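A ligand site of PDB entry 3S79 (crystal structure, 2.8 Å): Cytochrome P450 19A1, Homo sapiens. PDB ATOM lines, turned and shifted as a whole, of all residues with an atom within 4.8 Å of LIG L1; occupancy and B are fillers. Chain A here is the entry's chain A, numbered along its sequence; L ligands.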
ATOM      1  N   MET A 107      19.198  37.642 -27.213  1.00  0.00           N
ATOM      2  CA  MET A 107      18.529  37.206 -25.983  1.00  0.00           C
ATOM      3  C   MET A 107      17.901  38.368 -25.219  1.00  0.00           C
ATOM      4  O   MET A 107      16.968  38.186 -24.432  1.00  0.00           O
ATOM      5  CB  MET A 107      19.480  36.436 -25.066  1.00  0.00           C
ATOM      6  CG  MET A 107      20.356  35.429 -25.790  1.00  0.00           C
ATOM      7  SD  MET A 107      20.955  34.043 -24.801  1.00  0.00           S
ATOM      8  CE  MET A 107      21.857  34.863 -23.521  1.00  0.00           C
ATOM      9  N   ARG A 115      11.531  29.987 -30.692  1.00  0.00           N
ATOM     10  CA  ARG A 115      12.483  28.977 -31.172  1.00  0.00           C
ATOM     11  C   ARG A 115      11.971  28.531 -32.542  1.00  0.00           C
ATOM     12  O   ARG A 115      11.134  29.211 -33.141  1.00  0.00           O
ATOM     13  CB  ARG A 115      12.581  27.784 -30.217  1.00  0.00           C
ATOM     14  CG  ARG A 115      12.747  28.170 -28.768  1.00  0.00           C
ATOM     15  CD  ARG A 115      13.396  27.069 -27.951  1.00  0.00           C
ATOM     16  NE  ARG A 115      13.495  27.482 -26.552  1.00  0.00           N
ATOM     17  CZ  ARG A 115      14.488  28.214 -26.042  1.00  0.00           C
ATOM     18  NH1 ARG A 115      15.517  28.594 -26.801  1.00  0.00           N
ATOM     19  NH2 ARG A 115      14.472  28.553 -24.755  1.00  0.00           N
ATOM     20  N   ILE A 132       6.237  25.150 -23.013  1.00  0.00           N
ATOM     21  CA  ILE A 132       6.973  26.367 -23.250  1.00  0.00           C
ATOM     22  C   ILE A 132       8.279  26.161 -24.012  1.00  0.00           C
ATOM     23  O   ILE A 132       8.615  26.990 -24.859  1.00  0.00           O
ATOM     24  CB  ILE A 132       7.239  27.240 -21.978  1.00  0.00           C
ATOM     25  CG1 ILE A 132       8.044  26.496 -20.921  1.00  0.00           C
ATOM     26  CG2 ILE A 132       5.941  27.807 -21.412  1.00  0.00           C
ATOM     27  CD1 ILE A 132       8.785  27.477 -20.048  1.00  0.00           C
ATOM     28  N   ILE A 133       8.999  25.071 -23.714  1.00  0.00           N
ATOM     29  CA  ILE A 133      10.343  24.877 -24.263  1.00  0.00           C
ATOM     30  C   ILE A 133      10.383  25.171 -25.759  1.00  0.00           C
ATOM     31  O   ILE A 133      11.140  26.028 -26.200  1.00  0.00           O
ATOM     32  CB  ILE A 133      10.910  23.474 -23.965  1.00  0.00           C
ATOM     33  CG1 ILE A 133      10.803  23.147 -22.484  1.00  0.00           C
ATOM     34  CG2 ILE A 133      12.375  23.392 -24.382  1.00  0.00           C
ATOM     35  CD1 ILE A 133      11.091  21.687 -22.172  1.00  0.00           C
ATOM     36  N   TRP A 141       2.920  31.230 -25.488  1.00  0.00           N
ATOM     37  CA  TRP A 141       4.146  31.137 -24.705  1.00  0.00           C
ATOM     38  C   TRP A 141       4.157  32.199 -23.613  1.00  0.00           C
ATOM     39  O   TRP A 141       4.412  31.886 -22.439  1.00  0.00           O
ATOM     40  CB  TRP A 141       5.366  31.283 -25.622  1.00  0.00           C
ATOM     41  CG  TRP A 141       6.647  31.526 -24.883  1.00  0.00           C
ATOM     42  CD1 TRP A 141       7.426  30.598 -24.259  1.00  0.00           C
ATOM     43  CD2 TRP A 141       7.290  32.786 -24.702  1.00  0.00           C
ATOM     44  NE1 TRP A 141       8.523  31.202 -23.701  1.00  0.00           N
ATOM     45  CE2 TRP A 141       8.468  32.555 -23.959  1.00  0.00           C
ATOM     46  CE3 TRP A 141       6.988  34.098 -25.084  1.00  0.00           C
ATOM     47  CZ2 TRP A 141       9.338  33.583 -23.601  1.00  0.00           C
ATOM     48  CZ3 TRP A 141       7.850  35.108 -24.742  1.00  0.00           C
ATOM     49  CH2 TRP A 141       9.020  34.854 -23.995  1.00  0.00           C
ATOM     50  N   ARG A 145       4.573  30.818 -19.769  1.00  0.00           N
ATOM     51  CA  ARG A 145       5.830  31.014 -19.054  1.00  0.00           C
ATOM     52  C   ARG A 145       5.678  31.458 -17.575  1.00  0.00           C
ATOM     53  O   ARG A 145       6.388  30.941 -16.716  1.00  0.00           O
ATOM     54  CB  ARG A 145       6.768  31.939 -19.836  1.00  0.00           C
ATOM     55  CG  ARG A 145       8.172  31.962 -19.288  1.00  0.00           C
ATOM     56  CD  ARG A 145       9.152  32.540 -20.280  1.00  0.00           C
ATOM     57  NE  ARG A 145      10.308  33.117 -19.589  1.00  0.00           N
ATOM     58  CZ  ARG A 145      11.534  32.580 -19.552  1.00  0.00           C
ATOM     59  NH1 ARG A 145      11.794  31.431 -20.168  1.00  0.00           N
ATOM     60  NH2 ARG A 145      12.499  33.198 -18.888  1.00  0.00           N
ATOM     61  N   PHE A 148       5.766  28.734 -15.004  1.00  0.00           N
ATOM     62  CA  PHE A 148       7.080  28.129 -14.791  1.00  0.00           C
ATOM     63  C   PHE A 148       7.938  29.030 -13.929  1.00  0.00           C
ATOM     64  O   PHE A 148       8.578  28.548 -12.984  1.00  0.00           O
ATOM     65  CB  PHE A 148       7.764  27.830 -16.137  1.00  0.00           C
ATOM     66  CG  PHE A 148       7.250  26.590 -16.809  1.00  0.00           C
ATOM     67  CD1 PHE A 148       6.108  26.632 -17.609  1.00  0.00           C
ATOM     68  CD2 PHE A 148       7.900  25.372 -16.643  1.00  0.00           C
ATOM     69  CE1 PHE A 148       5.624  25.486 -18.234  1.00  0.00           C
ATOM     70  CE2 PHE A 148       7.425  24.215 -17.260  1.00  0.00           C
ATOM     71  CZ  PHE A 148       6.283  24.266 -18.057  1.00  0.00           C
ATOM     72  N   LEU A 152       9.663  28.164 -10.091  1.00  0.00           N
ATOM     73  CA  LEU A 152      11.127  27.998 -10.136  1.00  0.00           C
ATOM     74  C   LEU A 152      11.924  29.088  -9.385  1.00  0.00           C
ATOM     75  O   LEU A 152      13.148  29.165  -9.491  1.00  0.00           O
ATOM     76  CB  LEU A 152      11.600  27.874 -11.589  1.00  0.00           C
ATOM     77  CG  LEU A 152      11.126  26.631 -12.362  1.00  0.00           C
ATOM     78  CD1 LEU A 152      11.485  26.758 -13.823  1.00  0.00           C
ATOM     79  CD2 LEU A 152      11.678  25.352 -11.775  1.00  0.00           C
ATOM     80  N   PHE A 203       7.016  19.830  -7.638  1.00  0.00           N
ATOM     81  CA  PHE A 203       6.079  20.438  -8.606  1.00  0.00           C
ATOM     82  C   PHE A 203       4.749  19.740  -8.783  1.00  0.00           C
ATOM     83  O   PHE A 203       3.794  20.359  -9.263  1.00  0.00           O
ATOM     84  CB  PHE A 203       6.738  20.609  -9.978  1.00  0.00           C
ATOM     85  CG  PHE A 203       8.061  21.319  -9.934  1.00  0.00           C
ATOM     86  CD1 PHE A 203       8.140  22.631  -9.486  1.00  0.00           C
ATOM     87  CD2 PHE A 203       9.219  20.676 -10.365  1.00  0.00           C
ATOM     88  CE1 PHE A 203       9.367  23.297  -9.461  1.00  0.00           C
ATOM     89  CE2 PHE A 203      10.446  21.332 -10.342  1.00  0.00           C
ATOM     90  CZ  PHE A 203      10.524  22.642  -9.885  1.00  0.00           C
ATOM     91  N   MET A 303       7.873  20.118 -17.188  1.00  0.00           N
ATOM     92  CA  MET A 303       8.451  20.422 -15.891  1.00  0.00           C
ATOM     93  C   MET A 303       9.127  19.196 -15.269  1.00  0.00           C
ATOM     94  O   MET A 303      10.116  19.330 -14.562  1.00  0.00           O
ATOM     95  CB  MET A 303       7.379  20.987 -14.955  1.00  0.00           C
ATOM     96  CG  MET A 303       7.883  21.386 -13.567  1.00  0.00           C
ATOM     97  SD  MET A 303       9.091  22.740 -13.574  1.00  0.00           S
ATOM     98  CE  MET A 303       8.017  24.151 -13.332  1.00  0.00           C
ATOM     99  N   ALA A 306      12.638  18.193 -17.399  1.00  0.00           N
ATOM    100  CA  ALA A 306      13.678  19.214 -17.536  1.00  0.00           C
ATOM    101  C   ALA A 306      14.951  18.869 -16.762  1.00  0.00           C
ATOM    102  O   ALA A 306      16.029  18.817 -17.349  1.00  0.00           O
ATOM    103  CB  ALA A 306      13.147  20.584 -17.156  1.00  0.00           C
ATOM    104  N   ALA A 307      14.817  18.625 -15.459  1.00  0.00           N
ATOM    105  CA  ALA A 307      15.982  18.310 -14.634  1.00  0.00           C
ATOM    106  C   ALA A 307      16.620  16.951 -14.982  1.00  0.00           C
ATOM    107  O   ALA A 307      17.826  16.896 -15.227  1.00  0.00           O
ATOM    108  CB  ALA A 307      15.638  18.418 -13.154  1.00  0.00           C
ATOM    109  N   THR A 310      18.765  17.473 -18.253  1.00  0.00           N
ATOM    110  CA  THR A 310      19.932  18.352 -18.271  1.00  0.00           C
ATOM    111  C   THR A 310      20.797  18.318 -17.017  1.00  0.00           C
ATOM    112  O   THR A 310      22.017  18.290 -17.118  1.00  0.00           O
ATOM    113  CB  THR A 310      19.532  19.805 -18.553  1.00  0.00           C
ATOM    114  OG1 THR A 310      18.325  20.112 -17.829  1.00  0.00           O
ATOM    115  CG2 THR A 310      19.273  19.997 -20.027  1.00  0.00           C
ATOM    116  N   MET A 311      20.147  18.344 -15.852  1.00  0.00           N
ATOM    117  CA  MET A 311      20.864  18.386 -14.580  1.00  0.00           C
ATOM    118  C   MET A 311      21.742  17.167 -14.374  1.00  0.00           C
ATOM    119  O   MET A 311      22.880  17.279 -13.940  1.00  0.00           O
ATOM    120  CB  MET A 311      19.889  18.469 -13.418  1.00  0.00           C
ATOM    121  CG  MET A 311      19.194  19.798 -13.300  1.00  0.00           C
ATOM    122  SD  MET A 311      20.145  20.903 -12.273  1.00  0.00           S
ATOM    123  CE  MET A 311      20.180  19.967 -10.750  1.00  0.00           C
ATOM    124  N   SER A 314      24.702  17.070 -16.669  1.00  0.00           N
ATOM    125  CA  SER A 314      25.575  18.144 -16.165  1.00  0.00           C
ATOM    126  C   SER A 314      26.366  17.710 -14.946  1.00  0.00           C
ATOM    127  O   SER A 314      27.586  17.911 -14.886  1.00  0.00           O
ATOM    128  CB  SER A 314      24.763  19.374 -15.813  1.00  0.00           C
ATOM    129  OG  SER A 314      24.404  20.070 -16.980  1.00  0.00           O
ATOM    130  N   MET A 364      30.455  23.860 -16.618  1.00  0.00           N
ATOM    131  CA  MET A 364      29.490  24.204 -17.657  1.00  0.00           C
ATOM    132  C   MET A 364      30.138  24.916 -18.839  1.00  0.00           C
ATOM    133  O   MET A 364      29.797  24.616 -19.991  1.00  0.00           O
ATOM    134  CB  MET A 364      28.367  25.065 -17.094  1.00  0.00           C
ATOM    135  CG  MET A 364      27.350  24.278 -16.315  1.00  0.00           C
ATOM    136  SD  MET A 364      26.187  25.369 -15.489  1.00  0.00           S
ATOM    137  CE  MET A 364      25.079  25.734 -16.824  1.00  0.00           C
ATOM    138  N   VAL A 370      24.184  21.864 -22.659  1.00  0.00           N
ATOM    139  CA  VAL A 370      23.392  22.726 -23.518  1.00  0.00           C
ATOM    140  C   VAL A 370      24.300  23.769 -24.159  1.00  0.00           C
ATOM    141  O   VAL A 370      24.409  24.905 -23.702  1.00  0.00           O
ATOM    142  CB  VAL A 370      22.240  23.386 -22.741  1.00  0.00           C
ATOM    143  CG1 VAL A 370      21.260  24.021 -23.706  1.00  0.00           C
ATOM    144  CG2 VAL A 370      21.528  22.372 -21.859  1.00  0.00           C
ATOM    145  N   VAL A 373      21.614  27.198 -28.474  1.00  0.00           N
ATOM    146  CA  VAL A 373      20.269  27.737 -28.230  1.00  0.00           C
ATOM    147  C   VAL A 373      19.596  28.052 -29.552  1.00  0.00           C
ATOM    148  O   VAL A 373      20.175  28.721 -30.419  1.00  0.00           O
ATOM    149  CB  VAL A 373      20.328  29.011 -27.349  1.00  0.00           C
ATOM    150  CG1 VAL A 373      18.920  29.537 -27.072  1.00  0.00           C
ATOM    151  CG2 VAL A 373      21.040  28.732 -26.035  1.00  0.00           C
ATOM    152  N   ARG A 375      16.691  29.893 -31.725  1.00  0.00           N
ATOM    153  CA  ARG A 375      15.789  31.051 -31.741  1.00  0.00           C
ATOM    154  C   ARG A 375      15.224  31.342 -33.132  1.00  0.00           C
ATOM    155  O   ARG A 375      15.631  30.725 -34.127  1.00  0.00           O
ATOM    156  CB  ARG A 375      16.495  32.305 -31.183  1.00  0.00           C
ATOM    157  CG  ARG A 375      17.004  32.197 -29.750  1.00  0.00           C
ATOM    158  CD  ARG A 375      15.894  31.936 -28.749  1.00  0.00           C
ATOM    159  NE  ARG A 375      16.316  32.184 -27.366  1.00  0.00           N
ATOM    160  CZ  ARG A 375      16.165  33.348 -26.737  1.00  0.00           C
ATOM    161  NH1 ARG A 375      15.601  34.377 -27.359  1.00  0.00           N
ATOM    162  NH2 ARG A 375      16.565  33.491 -25.476  1.00  0.00           N
ATOM    163  N   ILE A 398      26.730  28.660 -28.054  1.00  0.00           N
ATOM    164  CA  ILE A 398      27.300  29.218 -26.827  1.00  0.00           C
ATOM    165  C   ILE A 398      28.535  28.453 -26.330  1.00  0.00           C
ATOM    166  O   ILE A 398      29.414  29.042 -25.701  1.00  0.00           O
ATOM    167  CB  ILE A 398      26.232  29.456 -25.736  1.00  0.00           C
ATOM    168  CG1 ILE A 398      25.573  28.146 -25.310  1.00  0.00           C
ATOM    169  CG2 ILE A 398      25.177  30.448 -26.253  1.00  0.00           C
ATOM    170  CD1 ILE A 398      24.718  28.245 -24.050  1.00  0.00           C
ATOM    171  N   PRO A 429      25.660  30.474 -19.742  1.00  0.00           N
ATOM    172  CA  PRO A 429      25.366  29.047 -19.678  1.00  0.00           C
ATOM    173  C   PRO A 429      23.852  28.739 -19.656  1.00  0.00           C
ATOM    174  O   PRO A 429      23.451  27.641 -20.033  1.00  0.00           O
ATOM    175  CB  PRO A 429      26.006  28.628 -18.365  1.00  0.00           C
ATOM    176  CG  PRO A 429      26.011  29.845 -17.523  1.00  0.00           C
ATOM    177  CD  PRO A 429      26.188  30.998 -18.476  1.00  0.00           C
ATOM    178  N   PHE A 430      23.038  29.691 -19.230  1.00  0.00           N
ATOM    179  CA  PHE A 430      21.601  29.482 -19.124  1.00  0.00           C
ATOM    180  C   PHE A 430      20.784  30.301 -20.111  1.00  0.00           C
ATOM    181  O   PHE A 430      19.588  30.057 -20.284  1.00  0.00           O
ATOM    182  CB  PHE A 430      21.120  29.815 -17.722  1.00  0.00           C
ATOM    183  CG  PHE A 430      21.691  28.932 -16.648  1.00  0.00           C
ATOM    184  CD1 PHE A 430      22.688  29.397 -15.813  1.00  0.00           C
ATOM    185  CD2 PHE A 430      21.205  27.645 -16.460  1.00  0.00           C
ATOM    186  CE1 PHE A 430      23.210  28.589 -14.806  1.00  0.00           C
ATOM    187  CE2 PHE A 430      21.718  26.827 -15.457  1.00  0.00           C
ATOM    188  CZ  PHE A 430      22.725  27.304 -14.628  1.00  0.00           C
ATOM    189  N   GLY A 431      21.415  31.272 -20.762  1.00  0.00           N
ATOM    190  CA  GLY A 431      20.677  32.314 -21.457  1.00  0.00           C
ATOM    191  C   GLY A 431      20.154  33.330 -20.442  1.00  0.00           C
ATOM    192  O   GLY A 431      20.102  33.044 -19.235  1.00  0.00           O
ATOM    193  N   PHE A 432      19.770  34.505 -20.928  1.00  0.00           N
ATOM    194  CA  PHE A 432      19.180  35.556 -20.075  1.00  0.00           C
ATOM    195  C   PHE A 432      18.063  36.224 -20.888  1.00  0.00           C
ATOM    196  O   PHE A 432      17.785  35.816 -22.000  1.00  0.00           O
ATOM    197  CB  PHE A 432      20.256  36.565 -19.653  1.00  0.00           C
ATOM    198  CG  PHE A 432      20.574  37.573 -20.725  1.00  0.00           C
ATOM    199  CD1 PHE A 432      19.966  38.834 -20.721  1.00  0.00           C
ATOM    200  CD2 PHE A 432      21.450  37.263 -21.757  1.00  0.00           C
ATOM    201  CE1 PHE A 432      20.231  39.759 -21.725  1.00  0.00           C
ATOM    202  CE2 PHE A 432      21.717  38.181 -22.773  1.00  0.00           C
ATOM    203  CZ  PHE A 432      21.098  39.427 -22.753  1.00  0.00           C
ATOM    204  N   ARG A 435      13.369  35.153 -22.653  1.00  0.00           N
ATOM    205  CA  ARG A 435      13.249  33.708 -22.910  1.00  0.00           C
ATOM    206  C   ARG A 435      14.489  32.914 -22.462  1.00  0.00           C
ATOM    207  O   ARG A 435      14.756  31.837 -22.986  1.00  0.00           O
ATOM    208  CB  ARG A 435      12.906  33.448 -24.384  1.00  0.00           C
ATOM    209  CG  ARG A 435      12.538  32.012 -24.680  1.00  0.00           C
ATOM    210  CD  ARG A 435      11.605  31.865 -25.852  1.00  0.00           C
ATOM    211  NE  ARG A 435      11.006  30.532 -25.810  1.00  0.00           N
ATOM    212  CZ  ARG A 435       9.988  30.107 -26.564  1.00  0.00           C
ATOM    213  NH1 ARG A 435       9.426  30.895 -27.465  1.00  0.00           N
ATOM    214  NH2 ARG A 435       9.533  28.872 -26.411  1.00  0.00           N
ATOM    215  N   GLY A 436      15.227  33.422 -21.472  1.00  0.00           N
ATOM    216  CA  GLY A 436      16.363  32.694 -20.912  1.00  0.00           C
ATOM    217  C   GLY A 436      15.856  31.522 -20.074  1.00  0.00           C
ATOM    218  O   GLY A 436      14.659  31.475 -19.751  1.00  0.00           O
ATOM    219  N   CYS A 437      16.743  30.591 -19.732  1.00  0.00           N
ATOM    220  CA  CYS A 437      16.357  29.399 -18.983  1.00  0.00           C
ATOM    221  C   CYS A 437      15.418  29.758 -17.840  1.00  0.00           C
ATOM    222  O   CYS A 437      15.730  30.641 -17.048  1.00  0.00           O
ATOM    223  CB  CYS A 437      17.582  28.677 -18.414  1.00  0.00           C
ATOM    224  SG  CYS A 437      17.180  27.275 -17.368  1.00  0.00           S
ATOM    225  N   ALA A 438      14.284  29.076 -17.768  1.00  0.00           N
ATOM    226  CA  ALA A 438      13.318  29.329 -16.707  1.00  0.00           C
ATOM    227  C   ALA A 438      13.847  28.850 -15.356  1.00  0.00           C
ATOM    228  O   ALA A 438      13.491  29.375 -14.308  1.00  0.00           O
ATOM    229  CB  ALA A 438      11.999  28.665 -17.019  1.00  0.00           C
ATOM    230  N   GLY A 439      14.707  27.837 -15.400  1.00  0.00           N
ATOM    231  CA  GLY A 439      15.226  27.245 -14.182  1.00  0.00           C
ATOM    232  C   GLY A 439      16.599  27.756 -13.822  1.00  0.00           C
ATOM    233  O   GLY A 439      17.251  27.187 -12.940  1.00  0.00           O
ATOM    234  N   ALA A 443      18.454  25.912 -10.702  1.00  0.00           N
ATOM    235  CA  ALA A 443      19.434  24.957 -11.187  1.00  0.00           C
ATOM    236  C   ALA A 443      20.729  25.041 -10.384  1.00  0.00           C
ATOM    237  O   ALA A 443      21.274  24.014  -9.981  1.00  0.00           O
ATOM    238  CB  ALA A 443      19.689  25.162 -12.667  1.00  0.00           C
ATOM    239  N   MET A 446      20.134  23.549  -6.933  1.00  0.00           N
ATOM    240  CA  MET A 446      20.067  22.092  -7.002  1.00  0.00           C
ATOM    241  C   MET A 446      21.432  21.459  -7.196  1.00  0.00           C
ATOM    242  O   MET A 446      21.781  20.505  -6.490  1.00  0.00           O
ATOM    243  CB  MET A 446      19.146  21.666  -8.131  1.00  0.00           C
ATOM    244  CG  MET A 446      17.694  21.905  -7.839  1.00  0.00           C
ATOM    245  SD  MET A 446      16.633  21.226  -9.117  1.00  0.00           S
ATOM    246  CE  MET A 446      16.668  22.574 -10.280  1.00  0.00           C
ATOM    247  N   MET A 447      22.208  21.986  -8.135  1.00  0.00           N
ATOM    248  CA  MET A 447      23.526  21.443  -8.413  1.00  0.00           C
ATOM    249  C   MET A 447      24.460  21.546  -7.231  1.00  0.00           C
ATOM    250  O   MET A 447      25.255  20.631  -6.985  1.00  0.00           O
ATOM    251  CB  MET A 447      24.152  22.090  -9.634  1.00  0.00           C
ATOM    252  CG  MET A 447      23.693  21.429 -10.909  1.00  0.00           C
ATOM    253  SD  MET A 447      24.399  22.145 -12.375  1.00  0.00           S
ATOM    254  CE  MET A 447      23.584  23.753 -12.424  1.00  0.00           C
HETATM  255  C1  LIG L   1      15.676  26.762 -21.406  1.00  0.00           C
HETATM  256  C2  LIG L   1      20.137  25.695 -19.858  1.00  0.00           C
HETATM  257  C3  LIG L   1      18.198  23.489 -16.029  1.00  0.00           C
HETATM  258  C4  LIG L   1      13.751  24.651 -17.459  1.00  0.00           C
HETATM  259  C5  LIG L   1      17.049  26.707 -21.306  1.00  0.00           C
HETATM  260  C6  LIG L   1      17.986  27.342 -22.204  1.00  0.00           C
HETATM  261  C7  LIG L   1      19.218  27.057 -21.770  1.00  0.00           C
HETATM  262  C8  LIG L   1      19.100  26.224 -20.585  1.00  0.00           C
HETATM  263  C9  LIG L   1      20.553  27.516 -22.411  1.00  0.00           C
HETATM  264  C10 LIG L   1      17.621  28.227 -23.426  1.00  0.00           C
HETATM  265  C11 LIG L   1      17.407  29.645 -22.924  1.00  0.00           C
HETATM  266  C12 LIG L   1      17.377  30.657 -24.044  1.00  0.00           C
HETATM  267  O1  LIG L   1      16.721  30.412 -25.104  1.00  0.00           O
HETATM  268  O2  LIG L   1      18.001  31.746 -23.888  1.00  0.00           O
HETATM  269  C13 LIG L   1      20.003  24.909 -18.745  1.00  0.00           C
HETATM  270  C14 LIG L   1      21.039  24.146 -18.077  1.00  0.00           C
HETATM  271  C15 LIG L   1      20.487  23.545 -17.014  1.00  0.00           C
HETATM  272  C16 LIG L   1      19.094  23.909 -16.996  1.00  0.00           C
HETATM  273  C17 LIG L   1      22.516  24.069 -18.512  1.00  0.00           C
HETATM  274  C18 LIG L   1      21.132  22.611 -15.957  1.00  0.00           C
HETATM  275  C19 LIG L   1      22.426  22.683 -15.644  1.00  0.00           C
HETATM  276  C20 LIG L   1      16.843  23.641 -16.061  1.00  0.00           C
HETATM  277  C21 LIG L   1      15.924  23.185 -15.043  1.00  0.00           C
HETATM  278  C22 LIG L   1      14.676  23.500 -15.440  1.00  0.00           C
HETATM  279  C23 LIG L   1      14.793  24.171 -16.718  1.00  0.00           C
HETATM  280  C24 LIG L   1      16.343  22.452 -13.747  1.00  0.00           C
HETATM  281  C25 LIG L   1      13.341  23.236 -14.707  1.00  0.00           C
HETATM  282  C26 LIG L   1      13.131  22.142 -13.960  1.00  0.00           C
HETATM  283  C27 LIG L   1      13.834  25.274 -18.680  1.00  0.00           C
HETATM  284  C28 LIG L   1      12.704  25.661 -19.493  1.00  0.00           C
HETATM  285  C29 LIG L   1      13.301  26.322 -20.734  1.00  0.00           C
HETATM  286  C30 LIG L   1      14.734  26.268 -20.535  1.00  0.00           C
HETATM  287  C31 LIG L   1      11.214  25.442 -19.156  1.00  0.00           C
HETATM  288  C32 LIG L   1      12.506  26.933 -21.917  1.00  0.00           C
HETATM  289  C33 LIG L   1      12.348  28.418 -21.621  1.00  0.00           C
HETATM  290  C34 LIG L   1      11.511  29.144 -22.654  1.00  0.00           C
HETATM  291  O3  LIG L   1      10.716  30.037 -22.274  1.00  0.00           O
HETATM  292  O4  LIG L   1      11.649  28.839 -23.871  1.00  0.00           O
HETATM  293  N1  LIG L   1      17.755  26.054 -20.316  1.00  0.00           N
HETATM  294  N2  LIG L   1      18.827  24.742 -18.057  1.00  0.00           N
HETATM  295  N3  LIG L   1      16.130  24.265 -17.059  1.00  0.00           N
HETATM  296  N4  LIG L   1      15.012  25.645 -19.314  1.00  0.00           N
HETATM  297 FE1  LIG L   1      16.956  25.209 -18.653  1.00  0.00          FE
HETATM  298  C1  LG2 L   2      15.000  22.210 -21.918  1.00  0.00           C
HETATM  299  C2  LG2 L   2      16.407  22.078 -22.528  1.00  0.00           C
HETATM  300  C3  LG2 L   2      15.930  24.103 -24.006  1.00  0.00           C
HETATM  301  C4  LG2 L   2      15.906  24.673 -25.425  1.00  0.00           C
HETATM  302  C5  LG2 L   2      17.284  24.495 -26.029  1.00  0.00           C
HETATM  303  C6  LG2 L   2      17.573  22.989 -26.112  1.00  0.00           C
HETATM  304  C7  LG2 L   2      18.726  22.859 -27.106  1.00  0.00           C
HETATM  305  C8  LG2 L   2      18.344  23.847 -28.210  1.00  0.00           C
HETATM  306  C9  LG2 L   2      17.458  24.844 -27.489  1.00  0.00           C
HETATM  307  C10 LG2 L   2      18.338  25.289 -25.250  1.00  0.00           C
HETATM  308  C11 LG2 L   2      17.414  22.859 -21.674  1.00  0.00           C
HETATM  309  C12 LG2 L   2      14.759  21.265 -20.741  1.00  0.00           C
HETATM  310  C13 LG2 L   2      15.060  19.869 -21.220  1.00  0.00           C
HETATM  311  C14 LG2 L   2      16.157  19.626 -21.988  1.00  0.00           C
HETATM  312  C15 LG2 L   2      16.835  20.604 -22.613  1.00  0.00           C
HETATM  313  C16 LG2 L   2      18.046  20.229 -23.436  1.00  0.00           C
HETATM  314  C17 LG2 L   2      17.907  20.836 -24.836  1.00  0.00           C
HETATM  315  C18 LG2 L   2      17.658  22.333 -24.741  1.00  0.00           C
HETATM  316  C19 LG2 L   2      16.366  22.630 -23.965  1.00  0.00           C
HETATM  317  O1  LG2 L   2      14.297  18.958 -20.896  1.00  0.00           O
HETATM  318  O2  LG2 L   2      16.949  25.822 -28.016  1.00  0.00           O
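The side-chain sulfur of Cys 437 binds an iron atom (FE1) of LIG L1, 2.4 Å away.
O4 of LIG L1 lies within salt-bridge range of NE of Arg 435, 2.7 Å away.
NH1 of Arg 145 lies within salt-bridge range of O3 of LIG L1.
NH2 of Arg 375 is in salt-bridge range of O2 of LIG L1, at 2.8 Å.
NH1 of Arg 115 is in salt-bridge range of O1 of LIG L1.
An oxygen (O3) of LIG L1 sits at hydrogen-bond distance from the indole nitrogen of Trp 141, at 2.9 Å.
NH1 of Arg 115 is in hydrogen-bond range of O2 of LG2 L2 (3.3 Å).
The backbone carbonyl oxygen of Phe 430 lies within hydrogen-bond range of the backbone NH of Cys 437, at 2.9 Å.
N of Gly 439 lies close to SG of Cys 437, at 3.2 Å.
O of Arg 435 is in hydrogen-bond range of NH2 of Arg 375 (3.5 Å).
The guanidinium group of Arg 435 is in hydrogen-bond range of the backbone carbonyl oxygen of Ile 132 (2.6 Å).
The backbone carbonyl oxygen (O) of Ile 133 lies within hydrogen-bond range of the guanidinium group (NH2) of Arg 435.
The guanidinium group of Arg 145 is in hydrogen-bond range of the backbone carbonyl oxygen of Gly 436 (2.9 Å).
OG of Ser 314 sits at hydrogen-bond distance from O of Thr 310, 3.0 Å away.
O of Ala 306 is in hydrogen-bond range of OG1 of Thr 310.
Merely in contact with LIG L1: Val 373 (3.1 Å), Ile 132 (3.3 Å), Phe 430 (3.4 Å), Met 446 (3.5 Å), Met 364 (3.5 Å), Gly 436 (3.5 Å), Ser 314 (3.5 Å), Ala 306 (3.6 Å), Met 447 (3.6 Å), Gly 431 (3.7 Å), Ile 133 (3.7 Å), Pro 429 (3.8 Å), Val 370 (3.8 Å), Thr 310 (3.8 Å), Ala 438 (3.8 Å), Met 107 (3.9 Å), Gly 439 (3.9 Å), Met 311 (3.9 Å) and Leu 152 (3.98 Å).
Hydrophobic or aromatic side chains that line LIG L1: Met 107, Ile 132, Trp 141, Leu 152, Ala 306, Met 311, Met 364, Val 370, Val 373, Phe 430, Ala 438, Met 446 and Met 447.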
